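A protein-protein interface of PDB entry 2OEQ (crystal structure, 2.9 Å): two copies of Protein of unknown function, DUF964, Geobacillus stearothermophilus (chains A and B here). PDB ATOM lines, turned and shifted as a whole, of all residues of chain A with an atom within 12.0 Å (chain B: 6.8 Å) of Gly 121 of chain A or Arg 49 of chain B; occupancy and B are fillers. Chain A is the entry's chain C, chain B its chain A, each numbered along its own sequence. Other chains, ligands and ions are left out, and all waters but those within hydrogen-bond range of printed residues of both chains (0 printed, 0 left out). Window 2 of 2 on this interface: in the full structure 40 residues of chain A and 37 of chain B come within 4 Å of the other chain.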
ATOM      1  N   GLU A 113     -19.325   4.292   2.239  1.00  0.00           N
ATOM      2  CA  GLU A 113     -20.215   3.737   3.253  1.00  0.00           C
ATOM      3  C   GLU A 113     -19.966   2.254   3.424  1.00  0.00           C
ATOM      4  O   GLU A 113     -19.914   1.760   4.548  1.00  0.00           O
ATOM      5  CB  GLU A 113     -21.678   3.983   2.864  1.00  0.00           C
ATOM      6  CG  GLU A 113     -22.198   5.397   3.145  1.00  0.00           C
ATOM      7  CD  GLU A 113     -23.402   5.762   2.276  1.00  0.00           C
ATOM      8  OE1 GLU A 113     -24.089   4.826   1.794  1.00  0.00           O
ATOM      9  OE2 GLU A 113     -23.657   6.979   2.082  1.00  0.00           O
ATOM     10  N   LEU A 114     -19.818   1.545   2.305  1.00  0.00           N
ATOM     11  CA  LEU A 114     -19.556   0.114   2.358  1.00  0.00           C
ATOM     12  C   LEU A 114     -18.166  -0.150   2.932  1.00  0.00           C
ATOM     13  O   LEU A 114     -17.977  -1.072   3.710  1.00  0.00           O
ATOM     14  CB  LEU A 114     -19.637  -0.505   0.972  1.00  0.00           C
ATOM     15  CG  LEU A 114     -19.574  -2.033   1.025  1.00  0.00           C
ATOM     16  CD1 LEU A 114     -21.003  -2.515   1.088  1.00  0.00           C
ATOM     17  CD2 LEU A 114     -18.818  -2.648  -0.194  1.00  0.00           C
ATOM     18  N   HIS A 115     -17.190   0.660   2.541  1.00  0.00           N
ATOM     19  CA  HIS A 115     -15.851   0.486   3.034  1.00  0.00           C
ATOM     20  C   HIS A 115     -15.877   0.497   4.517  1.00  0.00           C
ATOM     21  O   HIS A 115     -15.144  -0.269   5.154  1.00  0.00           O
ATOM     22  CB  HIS A 115     -14.936   1.599   2.560  1.00  0.00           C
ATOM     23  CG  HIS A 115     -14.285   1.308   1.252  1.00  0.00           C
ATOM     24  ND1 HIS A 115     -13.927   0.036   0.879  1.00  0.00           N
ATOM     25  CD2 HIS A 115     -13.937   2.121   0.227  1.00  0.00           C
ATOM     26  CE1 HIS A 115     -13.390   0.070  -0.328  1.00  0.00           C
ATOM     27  NE2 HIS A 115     -13.385   1.323  -0.744  1.00  0.00           N
ATOM     28  N   ARG A 116     -16.696   1.389   5.073  1.00  0.00           N
ATOM     29  CA  ARG A 116     -16.824   1.508   6.531  1.00  0.00           C
ATOM     30  C   ARG A 116     -17.285   0.184   7.158  1.00  0.00           C
ATOM     31  O   ARG A 116     -16.729  -0.276   8.157  1.00  0.00           O
ATOM     32  CB  ARG A 116     -17.805   2.625   6.891  1.00  0.00           C
ATOM     33  CG  ARG A 116     -18.066   2.727   8.378  1.00  0.00           C
ATOM     34  CD  ARG A 116     -18.415   4.147   8.789  1.00  0.00           C
ATOM     35  NE  ARG A 116     -18.596   4.298  10.235  1.00  0.00           N
ATOM     36  CZ  ARG A 116     -17.750   3.837  11.154  1.00  0.00           C
ATOM     37  NH1 ARG A 116     -18.000   4.036  12.441  1.00  0.00           N
ATOM     38  NH2 ARG A 116     -16.669   3.162  10.793  1.00  0.00           N
ATOM     39  N   SER A 117     -18.290  -0.428   6.548  1.00  0.00           N
ATOM     40  CA  SER A 117     -18.818  -1.675   7.032  1.00  0.00           C
ATOM     41  C   SER A 117     -17.766  -2.771   7.019  1.00  0.00           C
ATOM     42  O   SER A 117     -17.815  -3.694   7.821  1.00  0.00           O
ATOM     43  CB  SER A 117     -20.039  -2.069   6.205  1.00  0.00           C
ATOM     44  OG  SER A 117     -21.068  -1.110   6.396  1.00  0.00           O
ATOM     45  N   PHE A 118     -16.799  -2.689   6.120  1.00  0.00           N
ATOM     46  CA  PHE A 118     -15.748  -3.694   6.110  1.00  0.00           C
ATOM     47  C   PHE A 118     -15.039  -3.688   7.471  1.00  0.00           C
ATOM     48  O   PHE A 118     -14.353  -4.643   7.811  1.00  0.00           O
ATOM     49  CB  PHE A 118     -14.738  -3.406   4.997  1.00  0.00           C
ATOM     50  CG  PHE A 118     -15.271  -3.631   3.605  1.00  0.00           C
ATOM     51  CD1 PHE A 118     -16.606  -3.984   3.393  1.00  0.00           C
ATOM     52  CD2 PHE A 118     -14.429  -3.493   2.503  1.00  0.00           C
ATOM     53  CE1 PHE A 118     -17.103  -4.200   2.093  1.00  0.00           C
ATOM     54  CE2 PHE A 118     -14.909  -3.704   1.212  1.00  0.00           C
ATOM     55  CZ  PHE A 118     -16.259  -4.060   1.005  1.00  0.00           C
ATOM     56  N   MET A 119     -15.207  -2.613   8.246  1.00  0.00           N
ATOM     57  CA  MET A 119     -14.593  -2.522   9.572  1.00  0.00           C
ATOM     58  C   MET A 119     -15.432  -3.251  10.629  1.00  0.00           C
ATOM     59  O   MET A 119     -15.088  -3.230  11.820  1.00  0.00           O
ATOM     60  CB  MET A 119     -14.417  -1.062  10.025  1.00  0.00           C
ATOM     61  CG  MET A 119     -13.552  -0.192   9.127  1.00  0.00           C
ATOM     62  SD  MET A 119     -11.870  -0.985   8.622  1.00  0.00           S
ATOM     63  CE  MET A 119     -12.424  -1.533   6.876  1.00  0.00           C
ATOM     64  N   GLU A 120     -16.528  -3.884  10.193  1.00  0.00           N
ATOM     65  CA  GLU A 120     -17.430  -4.624  11.084  1.00  0.00           C
ATOM     66  C   GLU A 120     -16.729  -5.747  11.853  1.00  0.00           C
ATOM     67  O   GLU A 120     -16.542  -5.648  13.069  1.00  0.00           O
ATOM     68  CB  GLU A 120     -18.599  -5.204  10.289  1.00  0.00           C
ATOM     69  CG  GLU A 120     -19.399  -6.273  11.024  1.00  0.00           C
ATOM     70  CD  GLU A 120     -20.087  -5.766  12.280  1.00  0.00           C
ATOM     71  OE1 GLU A 120     -19.397  -5.290  13.210  1.00  0.00           O
ATOM     72  OE2 GLU A 120     -21.330  -5.856  12.338  1.00  0.00           O
ATOM     73  N   GLY A 121     -16.354  -6.809  11.147  1.00  0.00           N
ATOM     74  CA  GLY A 121     -15.672  -7.926  11.781  1.00  0.00           C
ATOM     75  C   GLY A 121     -15.980  -8.117  13.256  1.00  0.00           C
ATOM     76  O   GLY A 121     -15.317  -7.449  14.084  1.00  0.00           O
ATOM     77  N   TYR B  32     -20.319  -8.802  -0.414  1.00  0.00           N
ATOM     78  CA  TYR B  32     -19.825  -8.561   0.913  1.00  0.00           C
ATOM     79  C   TYR B  32     -20.526  -9.570   1.792  1.00  0.00           C
ATOM     80  O   TYR B  32     -19.883 -10.228   2.618  1.00  0.00           O
ATOM     81  CB  TYR B  32     -20.159  -7.167   1.429  1.00  0.00           C
ATOM     82  CG  TYR B  32     -19.626  -6.960   2.831  1.00  0.00           C
ATOM     83  CD1 TYR B  32     -20.229  -6.077   3.709  1.00  0.00           C
ATOM     84  CD2 TYR B  32     -18.470  -7.612   3.254  1.00  0.00           C
ATOM     85  CE1 TYR B  32     -19.691  -5.832   4.971  1.00  0.00           C
ATOM     86  CE2 TYR B  32     -17.927  -7.384   4.500  1.00  0.00           C
ATOM     87  CZ  TYR B  32     -18.537  -6.486   5.359  1.00  0.00           C
ATOM     88  OH  TYR B  32     -17.953  -6.207   6.585  1.00  0.00           O
ATOM     89  N   ARG B  36     -19.267 -12.190   4.557  1.00  0.00           N
ATOM     90  CA  ARG B  36     -19.663 -12.003   5.952  1.00  0.00           C
ATOM     91  C   ARG B  36     -20.381 -13.242   6.509  1.00  0.00           C
ATOM     92  O   ARG B  36     -20.191 -13.592   7.670  1.00  0.00           O
ATOM     93  CB  ARG B  36     -20.578 -10.788   6.078  1.00  0.00           C
ATOM     94  CG  ARG B  36     -20.269  -9.845   7.235  1.00  0.00           C
ATOM     95  CD  ARG B  36     -21.276  -8.689   7.223  1.00  0.00           C
ATOM     96  NE  ARG B  36     -20.828  -7.472   7.908  1.00  0.00           N
ATOM     97  CZ  ARG B  36     -21.510  -6.324   7.915  1.00  0.00           C
ATOM     98  NH1 ARG B  36     -22.672  -6.234   7.273  1.00  0.00           N
ATOM     99  NH2 ARG B  36     -21.035  -5.260   8.557  1.00  0.00           N
ATOM    100  N   TYR B  42     -14.994 -15.017   6.024  1.00  0.00           N
ATOM    101  CA  TYR B  42     -15.009 -13.798   6.810  1.00  0.00           C
ATOM    102  C   TYR B  42     -13.857 -13.799   7.796  1.00  0.00           C
ATOM    103  O   TYR B  42     -13.730 -12.890   8.618  1.00  0.00           O
ATOM    104  CB  TYR B  42     -16.329 -13.644   7.567  1.00  0.00           C
ATOM    105  CG  TYR B  42     -16.602 -12.230   8.052  1.00  0.00           C
ATOM    106  CD1 TYR B  42     -17.649 -11.957   8.934  1.00  0.00           C
ATOM    107  CD2 TYR B  42     -15.831 -11.163   7.608  1.00  0.00           C
ATOM    108  CE1 TYR B  42     -17.922 -10.646   9.361  1.00  0.00           C
ATOM    109  CE2 TYR B  42     -16.093  -9.857   8.024  1.00  0.00           C
ATOM    110  CZ  TYR B  42     -17.140  -9.603   8.895  1.00  0.00           C
ATOM    111  OH  TYR B  42     -17.411  -8.302   9.262  1.00  0.00           O
ATOM    112  N   ARG B  43     -13.033 -14.840   7.731  1.00  0.00           N
ATOM    113  CA  ARG B  43     -11.870 -14.949   8.599  1.00  0.00           C
ATOM    114  C   ARG B  43     -10.785 -14.291   7.771  1.00  0.00           C
ATOM    115  O   ARG B  43     -10.355 -13.181   8.069  1.00  0.00           O
ATOM    116  CB  ARG B  43     -11.520 -16.422   8.859  1.00  0.00           C
ATOM    117  CG  ARG B  43     -10.316 -16.651   9.777  1.00  0.00           C
ATOM    118  CD  ARG B  43      -9.966 -18.137   9.924  1.00  0.00           C
ATOM    119  NE  ARG B  43     -11.082 -18.948  10.425  1.00  0.00           N
ATOM    120  CZ  ARG B  43     -11.687 -18.776  11.602  1.00  0.00           C
ATOM    121  NH1 ARG B  43     -12.693 -19.566  11.963  1.00  0.00           N
ATOM    122  NH2 ARG B  43     -11.293 -17.813  12.422  1.00  0.00           N
ATOM    123  N   MET B  44     -10.382 -14.971   6.700  1.00  0.00           N
ATOM    124  CA  MET B  44      -9.352 -14.478   5.791  1.00  0.00           C
ATOM    125  C   MET B  44      -9.512 -12.969   5.559  1.00  0.00           C
ATOM    126  O   MET B  44      -8.567 -12.198   5.739  1.00  0.00           O
ATOM    127  CB  MET B  44      -9.418 -15.245   4.463  1.00  0.00           C
ATOM    128  CG  MET B  44      -9.100 -16.737   4.567  1.00  0.00           C
ATOM    129  SD  MET B  44      -8.117 -17.343   3.001  1.00  0.00           S
ATOM    130  CE  MET B  44      -8.999 -19.017   2.578  1.00  0.00           C
ATOM    131  N   PHE B  45     -10.717 -12.555   5.181  1.00  0.00           N
ATOM    132  CA  PHE B  45     -11.018 -11.143   4.943  1.00  0.00           C
ATOM    133  C   PHE B  45     -10.545 -10.283   6.102  1.00  0.00           C
ATOM    134  O   PHE B  45      -9.756  -9.355   5.933  1.00  0.00           O
ATOM    135  CB  PHE B  45     -12.534 -10.978   4.735  1.00  0.00           C
ATOM    136  CG  PHE B  45     -13.039  -9.549   4.797  1.00  0.00           C
ATOM    137  CD1 PHE B  45     -13.198  -8.896   6.019  1.00  0.00           C
ATOM    138  CD2 PHE B  45     -13.398  -8.877   3.631  1.00  0.00           C
ATOM    139  CE1 PHE B  45     -13.712  -7.602   6.081  1.00  0.00           C
ATOM    140  CE2 PHE B  45     -13.911  -7.584   3.680  1.00  0.00           C
ATOM    141  CZ  PHE B  45     -14.069  -6.946   4.904  1.00  0.00           C
ATOM    142  N   ALA B  46     -11.027 -10.587   7.293  1.00  0.00           N
ATOM    143  CA  ALA B  46     -10.636  -9.788   8.436  1.00  0.00           C
ATOM    144  C   ALA B  46      -9.130  -9.783   8.604  1.00  0.00           C
ATOM    145  O   ALA B  46      -8.568  -8.782   9.023  1.00  0.00           O
ATOM    146  CB  ALA B  46     -11.299 -10.306   9.688  1.00  0.00           C
ATOM    147  N   ASN B  47      -8.481 -10.896   8.273  1.00  0.00           N
ATOM    148  CA  ASN B  47      -7.031 -10.995   8.411  1.00  0.00           C
ATOM    149  C   ASN B  47      -6.352  -9.973   7.511  1.00  0.00           C
ATOM    150  O   ASN B  47      -5.580  -9.143   7.984  1.00  0.00           O
ATOM    151  CB  ASN B  47      -6.549 -12.407   8.062  1.00  0.00           C
ATOM    152  CG  ASN B  47      -5.034 -12.526   8.076  1.00  0.00           C
ATOM    153  OD1 ASN B  47      -4.375 -12.043   8.997  1.00  0.00           O
ATOM    154  ND2 ASN B  47      -4.476 -13.181   7.057  1.00  0.00           N
ATOM    155  N   VAL B  48      -6.651 -10.047   6.217  1.00  0.00           N
ATOM    156  CA  VAL B  48      -6.109  -9.127   5.241  1.00  0.00           C
ATOM    157  C   VAL B  48      -6.391  -7.727   5.737  1.00  0.00           C
ATOM    158  O   VAL B  48      -5.482  -6.918   5.902  1.00  0.00           O
ATOM    159  CB  VAL B  48      -6.798  -9.292   3.893  1.00  0.00           C
ATOM    160  CG1 VAL B  48      -6.045  -8.457   2.831  1.00  0.00           C
ATOM    161  CG2 VAL B  48      -6.866 -10.780   3.516  1.00  0.00           C
ATOM    162  N   ARG B  49      -7.667  -7.451   5.976  1.00  0.00           N
ATOM    163  CA  ARG B  49      -8.114  -6.158   6.492  1.00  0.00           C
ATOM    164  C   ARG B  49      -7.262  -5.623   7.644  1.00  0.00           C
ATOM    165  O   ARG B  49      -6.903  -4.452   7.691  1.00  0.00           O
ATOM    166  CB  ARG B  49      -9.564  -6.265   6.983  1.00  0.00           C
ATOM    167  CG  ARG B  49     -10.076  -5.002   7.661  1.00  0.00           C
ATOM    168  CD  ARG B  49     -11.382  -5.243   8.400  1.00  0.00           C
ATOM    169  NE  ARG B  49     -11.195  -6.004   9.639  1.00  0.00           N
ATOM    170  CZ  ARG B  49     -12.178  -6.524  10.375  1.00  0.00           C
ATOM    171  NH1 ARG B  49     -13.448  -6.380  10.010  1.00  0.00           N
ATOM    172  NH2 ARG B  49     -11.877  -7.190  11.480  1.00  0.00           N
ATOM    173  N   ASP B  50      -6.946  -6.489   8.584  1.00  0.00           N
ATOM    174  CA  ASP B  50      -6.189  -6.057   9.727  1.00  0.00           C
ATOM    175  C   ASP B  50      -4.741  -5.755   9.370  1.00  0.00           C
ATOM    176  O   ASP B  50      -4.196  -4.735   9.813  1.00  0.00           O
ATOM    177  CB  ASP B  50      -6.302  -7.106  10.852  1.00  0.00           C
ATOM    178  CG  ASP B  50      -7.587  -6.938  11.715  1.00  0.00           C
ATOM    179  OD1 ASP B  50      -8.654  -6.553  11.190  1.00  0.00           O
ATOM    180  OD2 ASP B  50      -7.531  -7.212  12.935  1.00  0.00           O
ATOM    181  N   ILE B  51      -4.110  -6.600   8.554  1.00  0.00           N
ATOM    182  CA  ILE B  51      -2.722  -6.328   8.222  1.00  0.00           C
ATOM    183  C   ILE B  51      -2.686  -5.069   7.347  1.00  0.00           C
ATOM    184  O   ILE B  51      -1.741  -4.273   7.423  1.00  0.00           O
ATOM    185  CB  ILE B  51      -1.962  -7.578   7.540  1.00  0.00           C
ATOM    186  CG1 ILE B  51      -1.947  -7.461   6.026  1.00  0.00           C
ATOM    187  CG2 ILE B  51      -2.550  -8.910   7.974  1.00  0.00           C
ATOM    188  CD1 ILE B  51      -0.779  -6.629   5.515  1.00  0.00           C
ATOM    189  N   GLN B  52      -3.733  -4.859   6.552  1.00  0.00           N
ATOM    190  CA  GLN B  52      -3.782  -3.676   5.693  1.00  0.00           C
ATOM    191  C   GLN B  52      -3.916  -2.379   6.475  1.00  0.00           C
ATOM    192  O   GLN B  52      -3.225  -1.396   6.219  1.00  0.00           O
ATOM    193  CB  GLN B  52      -4.917  -3.795   4.685  1.00  0.00           C
ATOM    194  CG  GLN B  52      -4.620  -4.807   3.601  1.00  0.00           C
ATOM    195  CD  GLN B  52      -3.294  -4.548   2.879  1.00  0.00           C
ATOM    196  OE1 GLN B  52      -2.839  -5.380   2.095  1.00  0.00           O
ATOM    197  NE2 GLN B  52      -2.676  -3.394   3.133  1.00  0.00           N
ATOM    198  N   LEU B  53      -4.815  -2.375   7.439  1.00  0.00           N
ATOM    199  CA  LEU B  53      -5.014  -1.205   8.269  1.00  0.00           C
ATOM    200  C   LEU B  53      -3.753  -0.962   9.081  1.00  0.00           C
ATOM    201  O   LEU B  53      -3.367   0.174   9.303  1.00  0.00           O
ATOM    202  CB  LEU B  53      -6.177  -1.470   9.209  1.00  0.00           C
ATOM    203  CG  LEU B  53      -7.486  -0.774   8.938  1.00  0.00           C
ATOM    204  CD1 LEU B  53      -8.634  -1.739   9.141  1.00  0.00           C
ATOM    205  CD2 LEU B  53      -7.555   0.419   9.862  1.00  0.00           C
ATOM    206  N   ARG B  54      -3.127  -2.041   9.546  1.00  0.00           N
ATOM    207  CA  ARG B  54      -1.912  -1.933  10.340  1.00  0.00           C
ATOM    208  C   ARG B  54      -0.815  -1.243   9.531  1.00  0.00           C
ATOM    209  O   ARG B  54      -0.047  -0.453  10.063  1.00  0.00           O
ATOM    210  CB  ARG B  54      -1.435  -3.320  10.778  1.00  0.00           C
ATOM    211  CG  ARG B  54      -0.049  -3.316  11.399  1.00  0.00           C
ATOM    212  CD  ARG B  54       0.476  -4.722  11.651  1.00  0.00           C
ATOM    213  NE  ARG B  54       1.939  -4.760  11.691  1.00  0.00           N
ATOM    214  CZ  ARG B  54       2.696  -4.035  12.515  1.00  0.00           C
ATOM    215  NH1 ARG B  54       4.021  -4.145  12.467  1.00  0.00           N
ATOM    216  NH2 ARG B  54       2.135  -3.201  13.387  1.00  0.00           N
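The side-chain hydroxyl (OH) of Tyr 32 of chain B is in hydrogen-bond range of the backbone carbonyl oxygen (O) of Ser 117 of chain A. OE2 of Glu 120 of chain A lies within salt-bridge range of NH2 of Arg 36 of chain B (3.8 Å). The backbone carbonyl oxygen (O) of Phe 118 of chain A lies within hydrogen-bond range of the guanidinium group (NH1) of Arg 49 of chain B (2.9 Å). N of Gly 121 of chain A is in hydrogen-bond range of OH of Tyr 42 of chain B, at 2.6 Å. NH1 of Arg 49 of chain B lies close to N of Gly 121 of chain A (3.1 Å).
The side-chain hydroxyl (OH) of Tyr 32 of chain B is in hydrogen-bond range of the guanidinium group (NE) of Arg 36 of chain B (3.4 Å). OH of Tyr 42 of chain B is in hydrogen-bond range of OH of Tyr 32 of chain B. The side-chain carboxylate of Asp 50 of chain B lies within salt-bridge range of the guanidinium group of Arg 49 of chain B (3.0 Å).
Ser 117 of chain A touches Arg 36 of chain B. Tyr 32 of chain B touches Phe 118 of chain A (OH to CA, 3.4 Å). O of Phe 118 of chain A touches CE1 of Phe 45 of chain B, at 3.5 Å. Met 119 of chain A touches Arg 49 of chain B (C to NH1, 3.8 Å). Leu 53 of chain B touches Met 119 of chain A. Glu 120 of chain A touches Tyr 32 of chain B. OH of Tyr 42 of chain B touches CG of Glu 120 of chain A, 3.3 Å away. Glu 120 of chain A touches Arg 49 of chain B.
Of the printed residues of chain B, Phe 118 of chain A touches Tyr 32 (3.4 Å), Phe 45 (3.5 Å) and Arg 49 (2.9 Å). Printed residues of chain B within 4 Å of Met 119 of chain A: Arg 49 and Leu 53. Of the printed residues of chain A, Tyr 42 of chain B touches Glu 120 (3.3 Å) and Gly 121 (2.6 Å). Of the printed residues of chain A, Phe 45 of chain B touches Phe 118 (3.5 Å). No residue of chain A comes within 4 Å of Ala 46 of chain B. No residue of chain A comes within 4 Å of Asn 47 of chain B. Of the printed residues of chain A, Arg 49 of chain B touches Phe 118 (2.9 Å), Met 119 (3.8 Å), Glu 120 (3.8 Å) and Gly 121 (3.1 Å). Asp 50 of chain B touches none of the printed residues of chain A. No residue of chain A comes within 4 Å of Ile 51 of chain B. No residue of chain A comes within 4 Å of Gln 52 of chain B. Leu 53 of chain B touches just one residue of chain A: Met 119 (3.4 Å). The nearest residue of chain B that does not touch Gly 121 of chain A is Tyr 32 of chain B (4.9 Å). The nearest printed residue of chain B that does not touch Met 119 of chain A is Tyr 32 of chain B (4.8 Å).
Of the 9 printed residues of chain A, 5 touch a printed residue of chain B. Hydrophobic or aromatic side chains of chain A that line the printed part of chain B: Phe 118 and Met 119. Along chain A the printed residues that touch a printed residue of chain B span positions 117 to 121. Hydrophobic or aromatic side chains of chain B within 4 Å of the printed part of chain A: Tyr 32, Tyr 42, Phe 45 and Leu 53. Among the printed residues, 13 pairs touch across the chains.
No position is printed for both chains. Of the 13 pairs that touch across the chains among the printed residues, none has its exchanged pair printed and touching as well.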
